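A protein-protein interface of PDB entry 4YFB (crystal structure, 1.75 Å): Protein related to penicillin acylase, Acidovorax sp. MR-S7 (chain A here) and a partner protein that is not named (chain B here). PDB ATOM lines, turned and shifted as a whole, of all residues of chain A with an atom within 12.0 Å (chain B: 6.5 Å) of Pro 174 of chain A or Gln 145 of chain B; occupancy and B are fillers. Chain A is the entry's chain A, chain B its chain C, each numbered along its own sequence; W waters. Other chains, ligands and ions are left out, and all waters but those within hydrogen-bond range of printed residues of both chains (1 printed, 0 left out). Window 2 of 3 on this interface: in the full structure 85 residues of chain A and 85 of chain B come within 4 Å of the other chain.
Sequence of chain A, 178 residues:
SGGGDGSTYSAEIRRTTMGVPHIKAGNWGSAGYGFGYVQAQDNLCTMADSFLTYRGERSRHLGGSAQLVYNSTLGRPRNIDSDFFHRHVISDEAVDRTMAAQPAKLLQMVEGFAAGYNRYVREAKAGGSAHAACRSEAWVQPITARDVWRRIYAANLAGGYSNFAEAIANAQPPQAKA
Gln 145 of chain B touches just one residue of chain A: Pro 174. No residue of chain A comes within 4 Å of Gln 85 of chain B. Of chain A, only Pro 174 comes within 4 Å of Ser 144 of chain B. No residue of chain A comes within 4 Å of Gly 146 of chain B. Printed residues of chain B within 4 Å of Gln 172 of chain A: Trp 143. Printed residues of chain B within 4 Å of Ala 171 of chain A: Trp 143 (3.9 Å). Printed residues of chain A within 4 Å of Pro 88 of chain B: Pro 174 (3.997 Å). Printed residues of chain B within 4 Å of Pro 173 of chain A: Trp 143. Glu 87 of chain B touches none of the printed residues of chain A. Asn 170 of chain A touches none of the printed residues of chain B. The nearest printed residue of chain B that does not touch Pro 174 of chain A is Leu 83 of chain B (5.7 Å). The nearest printed residue of chain B that does not touch Gln 172 of chain A is Ser 144 of chain B (6.6 Å).
OG of Ser 144 of chain B sits close to N of Gly 146 of chain B (3.2 Å). N of Thr 147 of chain B sits at hydrogen-bond distance from OG of Ser 144 of chain B, 3.0 Å away. O of Pro 88 of chain B is in hydrogen-bond range of NE1 of Trp 143 of chain B, at 2.9 Å.
Water W1 bridges the backbone carbonyl oxygen of Trp 143 of chain B (2.6 Å) and the backbone carbonyl oxygen of Gln 172 of chain A (2.8 Å).
C of Ala 171 of chain A touches CZ3 of Trp 143 of chain B (3.9 Å). Gln 172 of chain A touches Trp 143 of chain B. Trp 143 of chain B touches Pro 173 of chain A. Pro 174 of chain A touches Pro 88 of chain B. O of Trp 143 of chain B touches CD of Pro 174 of chain A, at 3.5 Å. CG of Pro 174 of chain A touches O of Ser 144 of chain B, at 3.5 Å. Pro 174 of chain A touches Gln 145 of chain B.
Of the 12 printed residues of chain B, 4 touch a printed residue of chain A. Hydrophobic or aromatic side chains of chain B that line the printed part of chain A: Pro 88 and Trp 143. Of the 5 printed residues of chain A, 4 touch a printed residue of chain B. Printed residues of chain A that touch a printed residue of chain B: Ala 171, Gln 172, Pro 173 and Pro 174. Among the printed residues, no Asp or Glu carboxylate lies within 4 Å of a Lys or Arg side-chain nitrogen of the other chain.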
ATOM      1  N   ASN A 170      -6.453  29.204   7.588  1.00  0.00           N
ATOM      2  CA  ASN A 170      -5.341  28.404   7.065  1.00  0.00           C
ATOM      3  C   ASN A 170      -5.584  27.479   5.834  1.00  0.00           C
ATOM      4  O   ASN A 170      -4.763  26.590   5.565  1.00  0.00           O
ATOM      5  CB  ASN A 170      -4.714  27.663   8.240  1.00  0.00           C
ATOM      6  CG  ASN A 170      -3.960  28.637   9.142  1.00  0.00           C
ATOM      7  OD1 ASN A 170      -2.822  28.940   8.860  1.00  0.00           O
ATOM      8  ND2 ASN A 170      -4.603  29.182  10.146  1.00  0.00           N
ATOM      9  N   ALA A 171      -6.687  27.692   5.116  1.00  0.00           N
ATOM     10  CA  ALA A 171      -7.005  26.935   3.875  1.00  0.00           C
ATOM     11  C   ALA A 171      -6.213  27.498   2.687  1.00  0.00           C
ATOM     12  O   ALA A 171      -6.399  28.643   2.285  1.00  0.00           O
ATOM     13  CB  ALA A 171      -8.512  26.934   3.586  1.00  0.00           C
ATOM     14  N   GLN A 172      -5.361  26.656   2.150  1.00  0.00           N
ATOM     15  CA  GLN A 172      -4.419  27.060   1.092  1.00  0.00           C
ATOM     16  C   GLN A 172      -4.298  25.902   0.133  1.00  0.00           C
ATOM     17  O   GLN A 172      -4.174  24.785   0.570  1.00  0.00           O
ATOM     18  CB  GLN A 172      -3.104  27.347   1.795  1.00  0.00           C
ATOM     19  CG  GLN A 172      -1.966  27.850   0.951  1.00  0.00           C
ATOM     20  CD  GLN A 172      -0.602  27.409   1.500  1.00  0.00           C
ATOM     21  OE1 GLN A 172      -0.389  26.218   1.798  1.00  0.00           O
ATOM     22  NE2 GLN A 172       0.352  28.359   1.577  1.00  0.00           N
ATOM     23  N   PRO A 173      -4.260  26.170  -1.205  1.00  0.00           N
ATOM     24  CA  PRO A 173      -4.023  25.096  -2.180  1.00  0.00           C
ATOM     25  C   PRO A 173      -2.577  24.559  -2.067  1.00  0.00           C
ATOM     26  O   PRO A 173      -1.727  25.255  -1.503  1.00  0.00           O
ATOM     27  CB  PRO A 173      -4.224  25.775  -3.548  1.00  0.00           C
ATOM     28  CG  PRO A 173      -4.326  27.233  -3.273  1.00  0.00           C
ATOM     29  CD  PRO A 173      -4.612  27.458  -1.826  1.00  0.00           C
ATOM     30  N   PRO A 174      -2.308  23.338  -2.558  1.00  0.00           N
ATOM     31  CA  PRO A 174      -0.923  22.800  -2.550  1.00  0.00           C
ATOM     32  C   PRO A 174      -0.148  23.406  -3.697  1.00  0.00           C
ATOM     33  O   PRO A 174      -0.684  24.329  -4.317  1.00  0.00           O
ATOM     34  CB  PRO A 174      -1.129  21.320  -2.829  1.00  0.00           C
ATOM     35  CG  PRO A 174      -2.350  21.290  -3.677  1.00  0.00           C
ATOM     36  CD  PRO A 174      -3.263  22.351  -3.097  1.00  0.00           C
ATOM     37  N   SER B  82     -14.377  18.371  -5.877  1.00  0.00           N
ATOM     38  CA  SER B  82     -13.522  17.593  -6.810  1.00  0.00           C
ATOM     39  C   SER B  82     -12.781  18.591  -7.705  1.00  0.00           C
ATOM     40  O   SER B  82     -13.423  19.370  -8.399  1.00  0.00           O
ATOM     41  CB  SER B  82     -14.361  16.654  -7.686  1.00  0.00           C
ATOM     42  OG  SER B  82     -15.146  15.841  -6.840  1.00  0.00           O
ATOM     43  N   LEU B  83     -11.454  18.606  -7.658  1.00  0.00           N
ATOM     44  CA  LEU B  83     -10.725  19.720  -8.232  1.00  0.00           C
ATOM     45  C   LEU B  83     -10.489  19.525  -9.731  1.00  0.00           C
ATOM     46  O   LEU B  83     -10.407  18.376 -10.170  1.00  0.00           O
ATOM     47  CB  LEU B  83      -9.426  19.913  -7.444  1.00  0.00           C
ATOM     48  CG  LEU B  83      -9.593  20.334  -5.966  1.00  0.00           C
ATOM     49  CD1 LEU B  83      -8.231  20.636  -5.347  1.00  0.00           C
ATOM     50  CD2 LEU B  83     -10.502  21.551  -5.897  1.00  0.00           C
ATOM     51  N   VAL B  84     -10.415  20.614 -10.509  1.00  0.00           N
ATOM     52  CA  VAL B  84     -10.083  20.512 -11.934  1.00  0.00           C
ATOM     53  C   VAL B  84      -8.596  20.179 -11.963  1.00  0.00           C
ATOM     54  O   VAL B  84      -7.807  20.960 -11.454  1.00  0.00           O
ATOM     55  CB  VAL B  84     -10.300  21.863 -12.633  1.00  0.00           C
ATOM     56  CG1 VAL B  84      -9.699  21.825 -14.062  1.00  0.00           C
ATOM     57  CG2 VAL B  84     -11.775  22.237 -12.617  1.00  0.00           C
ATOM     58  N   GLN B  85      -8.147  19.040 -12.514  1.00  0.00           N
ATOM     59  CA  GLN B  85      -6.736  18.776 -12.164  1.00  0.00           C
ATOM     60  C   GLN B  85      -5.741  19.778 -12.847  1.00  0.00           C
ATOM     61  O   GLN B  85      -6.055  20.526 -13.786  1.00  0.00           O
ATOM     62  CB  GLN B  85      -6.343  17.239 -12.065  1.00  0.00           C
ATOM     63  CG  GLN B  85      -5.232  16.667 -12.948  1.00  0.00           C
ATOM     64  CD  GLN B  85      -5.758  16.364 -14.327  1.00  0.00           C
ATOM     65  OE1 GLN B  85      -5.453  15.323 -14.946  1.00  0.00           O
ATOM     66  NE2 GLN B  85      -6.587  17.282 -14.824  1.00  0.00           N
ATOM     67  N   GLY B  86      -4.605  19.833 -12.191  1.00  0.00           N
ATOM     68  CA  GLY B  86      -3.561  20.868 -12.362  1.00  0.00           C
ATOM     69  C   GLY B  86      -3.940  22.288 -11.990  1.00  0.00           C
ATOM     70  O   GLY B  86      -3.161  23.223 -12.145  1.00  0.00           O
ATOM     71  N   GLU B  87      -5.139  22.456 -11.442  1.00  0.00           N
ATOM     72  CA  GLU B  87      -5.593  23.774 -11.165  1.00  0.00           C
ATOM     73  C   GLU B  87      -6.319  23.646  -9.841  1.00  0.00           C
ATOM     74  O   GLU B  87      -7.544  23.646  -9.830  1.00  0.00           O
ATOM     75  CB  GLU B  87      -6.551  24.223 -12.252  1.00  0.00           C
ATOM     76  CG  GLU B  87      -7.061  25.623 -12.012  1.00  0.00           C
ATOM     77  CD  GLU B  87      -7.670  26.246 -13.244  1.00  0.00           C
ATOM     78  OE1 GLU B  87      -8.693  26.940 -13.101  1.00  0.00           O
ATOM     79  OE2 GLU B  87      -7.122  26.079 -14.350  1.00  0.00           O
ATOM     80  N   PRO B  88      -5.556  23.491  -8.744  1.00  0.00           N
ATOM     81  CA  PRO B  88      -6.262  23.128  -7.533  1.00  0.00           C
ATOM     82  C   PRO B  88      -7.111  24.267  -6.904  1.00  0.00           C
ATOM     83  O   PRO B  88      -7.702  24.037  -5.840  1.00  0.00           O
ATOM     84  CB  PRO B  88      -5.142  22.616  -6.615  1.00  0.00           C
ATOM     85  CG  PRO B  88      -3.891  23.297  -7.103  1.00  0.00           C
ATOM     86  CD  PRO B  88      -4.086  23.526  -8.568  1.00  0.00           C
ATOM     87  N   TRP B 143      -6.198  19.755   1.553  1.00  0.00           N
ATOM     88  CA  TRP B 143      -6.450  20.255   0.215  1.00  0.00           C
ATOM     89  C   TRP B 143      -5.334  19.719  -0.662  1.00  0.00           C
ATOM     90  O   TRP B 143      -4.201  20.149  -0.558  1.00  0.00           O
ATOM     91  CB  TRP B 143      -6.470  21.785   0.302  1.00  0.00           C
ATOM     92  CG  TRP B 143      -6.815  22.548  -0.945  1.00  0.00           C
ATOM     93  CD1 TRP B 143      -6.762  22.112  -2.272  1.00  0.00           C
ATOM     94  CD2 TRP B 143      -7.296  23.929  -1.007  1.00  0.00           C
ATOM     95  NE1 TRP B 143      -7.143  23.106  -3.133  1.00  0.00           N
ATOM     96  CE2 TRP B 143      -7.500  24.229  -2.428  1.00  0.00           C
ATOM     97  CE3 TRP B 143      -7.603  24.920  -0.034  1.00  0.00           C
ATOM     98  CZ2 TRP B 143      -7.941  25.463  -2.865  1.00  0.00           C
ATOM     99  CZ3 TRP B 143      -8.046  26.165  -0.487  1.00  0.00           C
ATOM    100  CH2 TRP B 143      -8.204  26.433  -1.876  1.00  0.00           C
ATOM    101  N   SER B 144      -5.666  18.748  -1.509  1.00  0.00           N
ATOM    102  CA  SER B 144      -4.684  18.117  -2.404  1.00  0.00           C
ATOM    103  C   SER B 144      -4.794  18.648  -3.839  1.00  0.00           C
ATOM    104  O   SER B 144      -5.403  19.681  -4.091  1.00  0.00           O
ATOM    105  CB  SER B 144      -4.885  16.599  -2.393  1.00  0.00           C
ATOM    106  OG  SER B 144      -6.219  16.315  -2.757  1.00  0.00           O
ATOM    107  N   GLN B 145      -4.161  17.957  -4.794  1.00  0.00           N
ATOM    108  CA  GLN B 145      -4.420  18.223  -6.207  1.00  0.00           C
ATOM    109  C   GLN B 145      -5.823  17.789  -6.632  1.00  0.00           C
ATOM    110  O   GLN B 145      -6.346  18.260  -7.661  1.00  0.00           O
ATOM    111  CB  GLN B 145      -3.414  17.480  -7.106  1.00  0.00           C
ATOM    112  CG  GLN B 145      -1.973  17.579  -6.652  1.00  0.00           C
ATOM    113  CD  GLN B 145      -1.376  18.986  -6.800  1.00  0.00           C
ATOM    114  OE1 GLN B 145      -0.493  19.379  -6.024  1.00  0.00           O
ATOM    115  NE2 GLN B 145      -1.849  19.749  -7.792  1.00  0.00           N
ATOM    116  N   GLY B 146      -6.410  16.853  -5.880  1.00  0.00           N
ATOM    117  CA  GLY B 146      -7.699  16.242  -6.266  1.00  0.00           C
ATOM    118  C   GLY B 146      -8.913  16.720  -5.454  1.00  0.00           C
ATOM    119  O   GLY B 146     -10.041  16.708  -5.971  1.00  0.00           O
ATOM    120  N   THR B 147      -8.700  17.133  -4.197  1.00  0.00           N
ATOM    121  CA  THR B 147      -9.825  17.328  -3.318  1.00  0.00           C
ATOM    122  C   THR B 147      -9.587  18.552  -2.428  1.00  0.00           C
ATOM    123  O   THR B 147      -8.484  18.725  -1.923  1.00  0.00           O
ATOM    124  CB  THR B 147      -9.990  16.105  -2.385  1.00  0.00           C
ATOM    125  OG1 THR B 147     -10.203  14.944  -3.201  1.00  0.00           O
ATOM    126  CG2 THR B 147     -11.182  16.214  -1.579  1.00  0.00           C
HETATM  127  O   HOH W   1      -3.037  22.285   0.387  1.00  0.00           O
